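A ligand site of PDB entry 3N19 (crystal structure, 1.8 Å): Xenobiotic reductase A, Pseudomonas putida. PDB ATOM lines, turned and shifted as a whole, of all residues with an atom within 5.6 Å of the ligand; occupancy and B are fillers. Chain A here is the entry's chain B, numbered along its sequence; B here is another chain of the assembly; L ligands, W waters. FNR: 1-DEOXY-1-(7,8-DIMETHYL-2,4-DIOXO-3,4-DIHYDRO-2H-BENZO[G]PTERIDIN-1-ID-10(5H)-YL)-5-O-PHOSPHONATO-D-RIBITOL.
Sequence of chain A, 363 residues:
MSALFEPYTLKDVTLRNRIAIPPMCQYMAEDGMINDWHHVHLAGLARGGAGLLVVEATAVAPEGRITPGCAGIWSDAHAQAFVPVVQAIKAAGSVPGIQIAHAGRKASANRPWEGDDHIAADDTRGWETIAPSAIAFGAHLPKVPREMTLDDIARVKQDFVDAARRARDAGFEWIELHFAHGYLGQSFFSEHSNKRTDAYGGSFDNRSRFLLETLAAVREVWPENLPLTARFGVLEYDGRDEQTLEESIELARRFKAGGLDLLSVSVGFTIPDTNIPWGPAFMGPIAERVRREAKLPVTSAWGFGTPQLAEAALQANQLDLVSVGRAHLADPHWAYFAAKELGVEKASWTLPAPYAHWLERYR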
ATOM      1  N   PRO A  22      17.389  15.529 -17.933  1.00  0.00           N
ATOM      2  CA  PRO A  22      17.682  14.512 -18.966  1.00  0.00           C
ATOM      3  C   PRO A  22      19.149  14.135 -18.998  1.00  0.00           C
ATOM      4  O   PRO A  22      19.995  14.858 -18.416  1.00  0.00           O
ATOM      5  CB  PRO A  22      17.340  15.218 -20.270  1.00  0.00           C
ATOM      6  CG  PRO A  22      17.590  16.742 -19.952  1.00  0.00           C
ATOM      7  CD  PRO A  22      17.315  16.905 -18.478  1.00  0.00           C
ATOM      8  N   PRO A  23      19.495  13.065 -19.736  1.00  0.00           N
ATOM      9  CA  PRO A  23      20.911  12.701 -19.817  1.00  0.00           C
ATOM     10  C   PRO A  23      21.708  13.771 -20.512  1.00  0.00           C
ATOM     11  O   PRO A  23      21.338  14.180 -21.617  1.00  0.00           O
ATOM     12  CB  PRO A  23      20.922  11.397 -20.649  1.00  0.00           C
ATOM     13  CG  PRO A  23      19.512  11.522 -21.488  1.00  0.00           C
ATOM     14  CD  PRO A  23      18.608  12.088 -20.410  1.00  0.00           C
ATOM     15  N   MET A  24      22.816  14.194 -19.892  1.00  0.00           N
ATOM     16  CA  MET A  24      23.696  15.125 -20.533  1.00  0.00           C
ATOM     17  C   MET A  24      25.152  14.687 -20.432  1.00  0.00           C
ATOM     18  O   MET A  24      25.718  14.758 -19.338  1.00  0.00           O
ATOM     19  CB  MET A  24      23.510  16.487 -19.897  1.00  0.00           C
ATOM     20  CG  MET A  24      22.161  17.106 -20.219  1.00  0.00           C
ATOM     21  SD  MET A  24      22.092  18.813 -19.547  1.00  0.00           S
ATOM     22  CE  MET A  24      21.390  18.511 -17.943  1.00  0.00           C
ATOM     23  N   CYS A  25      25.713  14.255 -21.558  1.00  0.00           N
ATOM     24  CA  CYS A  25      27.103  13.840 -21.665  1.00  0.00           C
ATOM     25  C   CYS A  25      28.015  14.927 -21.082  1.00  0.00           C
ATOM     26  O   CYS A  25      27.808  16.067 -21.371  1.00  0.00           O
ATOM     27  CB  CYS A  25      27.490  13.708 -23.114  1.00  0.00           C
ATOM     28  SG  CYS A  25      26.899  12.087 -23.774  1.00  0.00           S
ATOM     29  N   GLN A  26      29.027  14.479 -20.371  1.00  0.00           N
ATOM     30  CA  GLN A  26      30.012  15.379 -19.710  1.00  0.00           C
ATOM     31  C   GLN A  26      31.377  15.302 -20.352  1.00  0.00           C
ATOM     32  O   GLN A  26      32.223  16.166 -20.125  1.00  0.00           O
ATOM     33  CB  GLN A  26      30.142  15.046 -18.246  1.00  0.00           C
ATOM     34  CG  GLN A  26      28.852  15.197 -17.489  1.00  0.00           C
ATOM     35  CD  GLN A  26      28.409  16.637 -17.421  1.00  0.00           C
ATOM     36  OE1 GLN A  26      29.016  17.441 -16.691  1.00  0.00           O
ATOM     37  NE2 GLN A  26      27.397  16.994 -18.220  1.00  0.00           N
ATOM     38  N   TYR A  27      31.611  14.219 -21.099  1.00  0.00           N
ATOM     39  CA  TYR A  27      32.845  14.003 -21.832  1.00  0.00           C
ATOM     40  C   TYR A  27      34.051  14.029 -20.884  1.00  0.00           C
ATOM     41  O   TYR A  27      35.141  14.436 -21.282  1.00  0.00           O
ATOM     42  CB  TYR A  27      32.999  15.022 -22.962  1.00  0.00           C
ATOM     43  CG  TYR A  27      31.746  15.151 -23.835  1.00  0.00           C
ATOM     44  CD1 TYR A  27      31.534  14.269 -24.897  1.00  0.00           C
ATOM     45  CD2 TYR A  27      30.779  16.152 -23.592  1.00  0.00           C
ATOM     46  CE1 TYR A  27      30.410  14.353 -25.706  1.00  0.00           C
ATOM     47  CE2 TYR A  27      29.627  16.245 -24.396  1.00  0.00           C
ATOM     48  CZ  TYR A  27      29.465  15.341 -25.474  1.00  0.00           C
ATOM     49  OH  TYR A  27      28.342  15.426 -26.282  1.00  0.00           O
ATOM     50  N   GLU A  56      23.905  10.580 -18.053  1.00  0.00           N
ATOM     51  CA  GLU A  56      24.267  10.748 -19.440  1.00  0.00           C
ATOM     52  C   GLU A  56      24.406   9.459 -20.213  1.00  0.00           C
ATOM     53  O   GLU A  56      24.700   8.417 -19.607  1.00  0.00           O
ATOM     54  CB  GLU A  56      25.617  11.428 -19.518  1.00  0.00           C
ATOM     55  CG  GLU A  56      26.777  10.590 -19.006  1.00  0.00           C
ATOM     56  CD  GLU A  56      28.022  11.449 -18.710  1.00  0.00           C
ATOM     57  OE1 GLU A  56      28.871  11.683 -19.613  1.00  0.00           O
ATOM     58  OE2 GLU A  56      28.107  11.933 -17.561  1.00  0.00           O
ATOM     59  N   ALA A  57      24.276   9.550 -21.550  1.00  0.00           N
ATOM     60  CA  ALA A  57      24.473   8.401 -22.460  1.00  0.00           C
ATOM     61  C   ALA A  57      25.712   7.628 -22.054  1.00  0.00           C
ATOM     62  O   ALA A  57      26.832   8.145 -22.176  1.00  0.00           O
ATOM     63  CB  ALA A  57      24.653   8.861 -23.877  1.00  0.00           C
ATOM     64  N   GLN A  99      20.877   6.471 -18.901  1.00  0.00           N
ATOM     65  CA  GLN A  99      20.640   6.263 -20.298  1.00  0.00           C
ATOM     66  C   GLN A  99      21.717   5.406 -20.914  1.00  0.00           C
ATOM     67  O   GLN A  99      22.879   5.799 -20.898  1.00  0.00           O
ATOM     68  CB  GLN A  99      20.610   7.588 -21.043  1.00  0.00           C
ATOM     69  CG  GLN A  99      20.217   7.383 -22.505  1.00  0.00           C
ATOM     70  CD  GLN A  99      20.398   8.662 -23.276  1.00  0.00           C
ATOM     71  OE1 GLN A  99      21.496   9.207 -23.273  1.00  0.00           O
ATOM     72  NE2 GLN A  99      19.319   9.147 -23.968  1.00  0.00           N
ATOM     73  N   GLU A 176      16.865   4.180 -19.464  1.00  0.00           N
ATOM     74  CA  GLU A 176      16.364   4.777 -20.676  1.00  0.00           C
ATOM     75  C   GLU A 176      17.183   4.222 -21.816  1.00  0.00           C
ATOM     76  O   GLU A 176      18.371   4.324 -21.836  1.00  0.00           O
ATOM     77  CB  GLU A 176      16.444   6.327 -20.618  1.00  0.00           C
ATOM     78  CG  GLU A 176      16.136   7.022 -21.949  1.00  0.00           C
ATOM     79  CD  GLU A 176      16.157   8.560 -21.849  1.00  0.00           C
ATOM     80  OE1 GLU A 176      15.367   9.158 -21.082  1.00  0.00           O
ATOM     81  OE2 GLU A 176      16.986   9.168 -22.550  1.00  0.00           O
ATOM     82  N   HIS A 178      18.622   4.551 -25.327  1.00  0.00           N
ATOM     83  CA  HIS A 178      18.881   5.691 -26.185  1.00  0.00           C
ATOM     84  C   HIS A 178      18.668   5.342 -27.647  1.00  0.00           C
ATOM     85  O   HIS A 178      19.615   4.998 -28.361  1.00  0.00           O
ATOM     86  CB  HIS A 178      20.303   6.257 -25.964  1.00  0.00           C
ATOM     87  CG  HIS A 178      20.489   7.614 -26.544  1.00  0.00           C
ATOM     88  ND1 HIS A 178      19.566   8.171 -27.398  1.00  0.00           N
ATOM     89  CD2 HIS A 178      21.468   8.541 -26.386  1.00  0.00           C
ATOM     90  CE1 HIS A 178      19.966   9.383 -27.753  1.00  0.00           C
ATOM     91  NE2 HIS A 178      21.110   9.644 -27.131  1.00  0.00           N
ATOM     92  N   HIS A 181      18.548  10.690 -31.637  1.00  0.00           N
ATOM     93  CA  HIS A 181      19.687  11.544 -32.010  1.00  0.00           C
ATOM     94  C   HIS A 181      20.671  11.048 -33.031  1.00  0.00           C
ATOM     95  O   HIS A 181      21.819  11.488 -33.031  1.00  0.00           O
ATOM     96  CB  HIS A 181      20.410  11.973 -30.734  1.00  0.00           C
ATOM     97  CG  HIS A 181      19.484  12.627 -29.760  1.00  0.00           C
ATOM     98  ND1 HIS A 181      19.789  12.807 -28.429  1.00  0.00           N
ATOM     99  CD2 HIS A 181      18.229  13.122 -29.930  1.00  0.00           C
ATOM    100  CE1 HIS A 181      18.761  13.386 -27.817  1.00  0.00           C
ATOM    101  NE2 HIS A 181      17.808  13.577 -28.710  1.00  0.00           N
ATOM    102  N   ARG A 231      14.309   6.919 -25.275  1.00  0.00           N
ATOM    103  CA  ARG A 231      14.282   8.204 -25.961  1.00  0.00           C
ATOM    104  C   ARG A 231      14.315   7.894 -27.448  1.00  0.00           C
ATOM    105  O   ARG A 231      15.099   7.062 -27.939  1.00  0.00           O
ATOM    106  CB  ARG A 231      15.502   9.045 -25.561  1.00  0.00           C
ATOM    107  CG  ARG A 231      15.408  10.467 -26.001  1.00  0.00           C
ATOM    108  CD  ARG A 231      16.355  11.405 -25.189  1.00  0.00           C
ATOM    109  NE  ARG A 231      15.743  12.749 -25.122  1.00  0.00           N
ATOM    110  CZ  ARG A 231      16.378  13.836 -24.669  1.00  0.00           C
ATOM    111  NH1 ARG A 231      17.635  13.719 -24.292  1.00  0.00           N
ATOM    112  NH2 ARG A 231      15.772  15.022 -24.608  1.00  0.00           N
ATOM    113  N   SER A 266      11.841  13.002 -28.794  1.00  0.00           N
ATOM    114  CA  SER A 266      12.853  13.936 -29.236  1.00  0.00           C
ATOM    115  C   SER A 266      12.900  14.071 -30.749  1.00  0.00           C
ATOM    116  O   SER A 266      11.959  13.717 -31.448  1.00  0.00           O
ATOM    117  CB  SER A 266      14.224  13.485 -28.673  1.00  0.00           C
ATOM    118  OG  SER A 266      15.200  14.499 -28.881  1.00  0.00           O
ATOM    119  N   ALA A 301      11.999  17.790 -24.060  1.00  0.00           N
ATOM    120  CA  ALA A 301      12.999  18.784 -23.701  1.00  0.00           C
ATOM    121  C   ALA A 301      13.129  19.790 -24.825  1.00  0.00           C
ATOM    122  O   ALA A 301      12.211  19.924 -25.662  1.00  0.00           O
ATOM    123  CB  ALA A 301      14.371  18.061 -23.478  1.00  0.00           C
ATOM    124  N   TRP A 302      14.254  20.477 -24.856  1.00  0.00           N
ATOM    125  CA  TRP A 302      14.639  21.327 -25.977  1.00  0.00           C
ATOM    126  C   TRP A 302      13.866  22.604 -25.914  1.00  0.00           C
ATOM    127  O   TRP A 302      13.420  23.084 -26.952  1.00  0.00           O
ATOM    128  CB  TRP A 302      14.352  20.668 -27.338  1.00  0.00           C
ATOM    129  CG  TRP A 302      15.037  19.375 -27.506  1.00  0.00           C
ATOM    130  CD1 TRP A 302      14.486  18.130 -27.443  1.00  0.00           C
ATOM    131  CD2 TRP A 302      16.420  19.178 -27.725  1.00  0.00           C
ATOM    132  NE1 TRP A 302      15.439  17.176 -27.627  1.00  0.00           N
ATOM    133  CE2 TRP A 302      16.647  17.806 -27.805  1.00  0.00           C
ATOM    134  CE3 TRP A 302      17.507  20.058 -27.881  1.00  0.00           C
ATOM    135  CZ2 TRP A 302      17.913  17.262 -28.023  1.00  0.00           C
ATOM    136  CZ3 TRP A 302      18.756  19.530 -28.097  1.00  0.00           C
ATOM    137  CH2 TRP A 302      18.948  18.146 -28.180  1.00  0.00           C
ATOM    138  N   GLY A 303      13.664  23.118 -24.711  1.00  0.00           N
ATOM    139  CA  GLY A 303      13.126  24.458 -24.540  1.00  0.00           C
ATOM    140  C   GLY A 303      12.070  24.676 -23.474  1.00  0.00           C
ATOM    141  O   GLY A 303      11.317  25.651 -23.578  1.00  0.00           O
ATOM    142  N   PHE A 304      11.972  23.781 -22.486  1.00  0.00           N
ATOM    143  CA  PHE A 304      10.982  23.944 -21.417  1.00  0.00           C
ATOM    144  C   PHE A 304      11.634  24.519 -20.198  1.00  0.00           C
ATOM    145  O   PHE A 304      11.052  24.564 -19.119  1.00  0.00           O
ATOM    146  CB  PHE A 304      10.284  22.619 -21.048  1.00  0.00           C
ATOM    147  CG  PHE A 304       9.461  22.020 -22.158  1.00  0.00           C
ATOM    148  CD1 PHE A 304       8.155  22.442 -22.376  1.00  0.00           C
ATOM    149  CD2 PHE A 304       9.986  21.021 -22.954  1.00  0.00           C
ATOM    150  CE1 PHE A 304       7.381  21.880 -23.396  1.00  0.00           C
ATOM    151  CE2 PHE A 304       9.229  20.457 -23.973  1.00  0.00           C
ATOM    152  CZ  PHE A 304       7.918  20.887 -24.194  1.00  0.00           C
ATOM    153  N   GLY A 305      12.849  24.991 -20.381  1.00  0.00           N
ATOM    154  CA  GLY A 305      13.638  25.433 -19.269  1.00  0.00           C
ATOM    155  C   GLY A 305      13.271  26.768 -18.658  1.00  0.00           C
ATOM    156  O   GLY A 305      14.160  27.436 -18.178  1.00  0.00           O
ATOM    157  N   SER A 323      11.631  17.602 -18.845  1.00  0.00           N
ATOM    158  CA  SER A 323      13.082  17.513 -18.759  1.00  0.00           C
ATOM    159  C   SER A 323      13.718  18.875 -18.931  1.00  0.00           C
ATOM    160  O   SER A 323      13.375  19.603 -19.831  1.00  0.00           O
ATOM    161  CB  SER A 323      13.566  16.561 -19.855  1.00  0.00           C
ATOM    162  OG  SER A 323      13.015  15.256 -19.600  1.00  0.00           O
ATOM    163  N   VAL A 324      14.657  19.219 -18.071  1.00  0.00           N
ATOM    164  CA  VAL A 324      15.266  20.539 -18.131  1.00  0.00           C
ATOM    165  C   VAL A 324      16.773  20.330 -18.109  1.00  0.00           C
ATOM    166  O   VAL A 324      17.285  19.876 -17.118  1.00  0.00           O
ATOM    167  CB  VAL A 324      14.797  21.385 -16.939  1.00  0.00           C
ATOM    168  CG1 VAL A 324      15.457  22.788 -16.923  1.00  0.00           C
ATOM    169  CG2 VAL A 324      13.272  21.501 -16.989  1.00  0.00           C
ATOM    170  N   GLY A 325      17.432  20.632 -19.218  1.00  0.00           N
ATOM    171  CA  GLY A 325      18.813  20.252 -19.427  1.00  0.00           C
ATOM    172  C   GLY A 325      19.760  21.400 -19.172  1.00  0.00           C
ATOM    173  O   GLY A 325      20.382  21.441 -18.129  1.00  0.00           O
ATOM    174  N   ARG A 326      19.889  22.333 -20.107  1.00  0.00           N
ATOM    175  CA  ARG A 326      20.904  23.362 -19.970  1.00  0.00           C
ATOM    176  C   ARG A 326      20.718  24.277 -18.747  1.00  0.00           C
ATOM    177  O   ARG A 326      21.700  24.707 -18.120  1.00  0.00           O
ATOM    178  CB  ARG A 326      21.050  24.171 -21.236  1.00  0.00           C
ATOM    179  CG  ARG A 326      21.689  23.372 -22.320  1.00  0.00           C
ATOM    180  CD  ARG A 326      21.560  24.059 -23.644  1.00  0.00           C
ATOM    181  NE  ARG A 326      20.167  24.055 -24.051  1.00  0.00           N
ATOM    182  CZ  ARG A 326      19.724  24.395 -25.258  1.00  0.00           C
ATOM    183  NH1 ARG A 326      20.580  24.794 -26.195  1.00  0.00           N
ATOM    184  NH2 ARG A 326      18.437  24.343 -25.531  1.00  0.00           N
ATOM    185  N   ALA A 327      19.471  24.595 -18.423  1.00  0.00           N
ATOM    186  CA  ALA A 327      19.158  25.339 -17.206  1.00  0.00           C
ATOM    187  C   ALA A 327      19.860  24.735 -15.958  1.00  0.00           C
ATOM    188  O   ALA A 327      20.312  25.477 -15.114  1.00  0.00           O
ATOM    189  CB  ALA A 327      17.682  25.450 -16.993  1.00  0.00           C
ATOM    190  N   LEU A 329      22.679  23.021 -15.945  1.00  0.00           N
ATOM    191  CA  LEU A 329      24.101  23.223 -16.078  1.00  0.00           C
ATOM    192  C   LEU A 329      24.372  24.645 -15.620  1.00  0.00           C
ATOM    193  O   LEU A 329      25.371  24.919 -14.977  1.00  0.00           O
ATOM    194  CB  LEU A 329      24.547  23.019 -17.519  1.00  0.00           C
ATOM    195  CG  LEU A 329      24.303  21.639 -18.125  1.00  0.00           C
ATOM    196  CD1 LEU A 329      24.751  21.718 -19.574  1.00  0.00           C
ATOM    197  CD2 LEU A 329      25.036  20.531 -17.415  1.00  0.00           C
ATOM    198  N   PRO B 354      32.670  21.340 -19.445  1.00  0.00           N
ATOM    199  CA  PRO B 354      31.448  20.553 -19.752  1.00  0.00           C
ATOM    200  C   PRO B 354      30.159  21.337 -19.541  1.00  0.00           C
ATOM    201  O   PRO B 354      29.079  20.929 -19.987  1.00  0.00           O
ATOM    202  CB  PRO B 354      31.488  19.407 -18.747  1.00  0.00           C
ATOM    203  CG  PRO B 354      32.944  19.227 -18.420  1.00  0.00           C
ATOM    204  CD  PRO B 354      33.486  20.676 -18.410  1.00  0.00           C
ATOM    205  N   TRP B 358      28.157  24.778 -23.599  1.00  0.00           N
ATOM    206  CA  TRP B 358      26.741  24.696 -23.971  1.00  0.00           C
ATOM    207  C   TRP B 358      25.999  25.942 -23.614  1.00  0.00           C
ATOM    208  O   TRP B 358      24.871  26.166 -24.067  1.00  0.00           O
ATOM    209  CB  TRP B 358      26.093  23.536 -23.203  1.00  0.00           C
ATOM    210  CG  TRP B 358      26.835  22.300 -23.459  1.00  0.00           C
ATOM    211  CD1 TRP B 358      27.627  21.613 -22.595  1.00  0.00           C
ATOM    212  CD2 TRP B 358      26.923  21.626 -24.732  1.00  0.00           C
ATOM    213  NE1 TRP B 358      28.191  20.525 -23.249  1.00  0.00           N
ATOM    214  CE2 TRP B 358      27.769  20.514 -24.553  1.00  0.00           C
ATOM    215  CE3 TRP B 358      26.369  21.867 -25.986  1.00  0.00           C
ATOM    216  CZ2 TRP B 358      28.050  19.636 -25.588  1.00  0.00           C
ATOM    217  CZ3 TRP B 358      26.661  21.001 -27.010  1.00  0.00           C
ATOM    218  CH2 TRP B 358      27.498  19.914 -26.810  1.00  0.00           C
HETATM  219  C9A FNR L   1      22.715  16.741 -24.223  1.00  0.00           C
HETATM  220  N10 FNR L   1      21.610  15.972 -24.590  1.00  0.00           N
HETATM  221  CAA FNR L   1      21.651  14.586 -24.573  1.00  0.00           C
HETATM  222  N1  FNR L   1      20.524  13.931 -24.776  1.00  0.00           N
HETATM  223  C2  FNR L   1      20.558  12.540 -24.726  1.00  0.00           C
HETATM  224  O2  FNR L   1      19.607  11.896 -25.162  1.00  0.00           O
HETATM  225  N3  FNR L   1      21.661  11.882 -24.192  1.00  0.00           N
HETATM  226  C4  FNR L   1      22.712  12.622 -23.769  1.00  0.00           C
HETATM  227  O4  FNR L   1      23.702  12.093 -23.262  1.00  0.00           O
HETATM  228  C4A FNR L   1      22.722  13.968 -24.119  1.00  0.00           C
HETATM  229  N5  FNR L   1      24.050  14.766 -23.908  1.00  0.00           N
HETATM  230  C5A FNR L   1      23.890  16.120 -23.755  1.00  0.00           C
HETATM  231  C6  FNR L   1      24.745  16.835 -22.917  1.00  0.00           C
HETATM  232  C7  FNR L   1      24.698  18.215 -22.940  1.00  0.00           C
HETATM  233  C7M FNR L   1      25.878  18.989 -22.404  1.00  0.00           C
HETATM  234  C8  FNR L   1      23.594  18.850 -23.467  1.00  0.00           C
HETATM  235  C8M FNR L   1      23.520  20.343 -23.506  1.00  0.00           C
HETATM  236  C9  FNR L   1      22.521  18.115 -23.943  1.00  0.00           C
HETATM  237  C1' FNR L   1      20.313  16.678 -24.899  1.00  0.00           C
HETATM  238  C2' FNR L   1      19.586  16.996 -23.574  1.00  0.00           C
HETATM  239  O2' FNR L   1      19.201  15.773 -22.946  1.00  0.00           O
HETATM  240  C3' FNR L   1      18.339  17.844 -23.812  1.00  0.00           C
HETATM  241  O3' FNR L   1      17.496  17.136 -24.690  1.00  0.00           O
HETATM  242  C4' FNR L   1      18.733  19.187 -24.428  1.00  0.00           C
HETATM  243  O4' FNR L   1      19.696  19.782 -23.566  1.00  0.00           O
HETATM  244  C5' FNR L   1      17.525  20.102 -24.653  1.00  0.00           C
HETATM  245  O5' FNR L   1      16.909  20.409 -23.424  1.00  0.00           O
HETATM  246  P   FNR L   1      17.188  21.883 -22.752  1.00  0.00           P
HETATM  247  O1P FNR L   1      18.663  22.041 -22.639  1.00  0.00           O
HETATM  248  O2P FNR L   1      16.552  22.973 -23.593  1.00  0.00           O
HETATM  249  O3P FNR L   1      16.429  21.812 -21.458  1.00  0.00           O
HETATM  250  O   HOH W   1      26.010  13.982 -25.977  1.00  0.00           O
HETATM  251  O   HOH W   2      17.007  24.072 -20.000  1.00  0.00           O
HETATM  252  O   HOH W   3      13.847  21.856 -21.875  1.00  0.00           O
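O3P of the ligand sits at hydrogen-bond distance from N of Gly 325 (2.7 Å). NH2 of Arg 231 sits at hydrogen-bond distance from O3' of the ligand (2.7 Å). The backbone NH (N) of Arg 326 lies within hydrogen-bond range of an oxygen (O1P) of the ligand, 2.8 Å away. The guanidinium group of Arg 326 is in salt-bridge range of an oxygen (O1P) of the ligand, 2.9 Å away. The side-chain amide oxygen (OE1) of Gln 99 sits at hydrogen-bond distance from a nitrogen (N3) of the ligand (2.8 Å). O of Pro 23 lies close to O2' of the ligand, at 3.0 Å. The backbone NH of Cys 25 lies close to an oxygen (O4) of the ligand. SG of Cys 25 lies within hydrogen-bond range of O4 of the ligand, at 3.2 Å. The backbone NH (N) of Trp 302 is in hydrogen-bond range of an oxygen (O5') of the ligand (3.0 Å). N of Gly 303 is in hydrogen-bond range of O2P of the ligand, 3.1 Å away. The backbone NH (N) of Ala 57 sits at hydrogen-bond distance from an oxygen (O4) of the ligand (3.1 Å). ND1 of His 181 sits close to O2 of the ligand. A ring nitrogen (NE2) of His 178 is in hydrogen-bond range of an oxygen (O2) of the ligand.
N of Ala 57 lies close to OE1 of Gln 99 (3.3 Å). The side-chain carboxylate of Glu 176 sits at hydrogen-bond distance from the side-chain amide nitrogen of Gln 99. NE1 of Trp 358 of chain B sits close to O of Pro 354 of chain B (3.4 Å). The indole nitrogen of Trp 302 is in hydrogen-bond range of the side-chain hydroxyl of Ser 266, 3.0 Å away. O of Met 24 is in hydrogen-bond range of NE2 of Gln 26 (3.0 Å). A ring nitrogen (NE2) of His 181 sits at hydrogen-bond distance from the side-chain hydroxyl of Ser 266.
Residues that only touch the ligand: Trp 358 of chain B (2.9 Å), Met 24 (3.1 Å), Pro 22 (3.3 Å), Ala 301 (3.5 Å) and Val 324 (3.7 Å). Of the 27 residues printed, 16 come within 4 Å of the ligand.
Water W2 lies within hydrogen-bond range of an oxygen (O3P) of the ligand (2.8 Å), the backbone NH of Ala 327 (3.0 Å) and the backbone NH of Arg 326 (3.4 Å). Water W1 lies within hydrogen-bond range of OH of Tyr 27 (2.8 Å), N5 of the ligand (3.0 Å) and SG of Cys 25 (3.0 Å).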
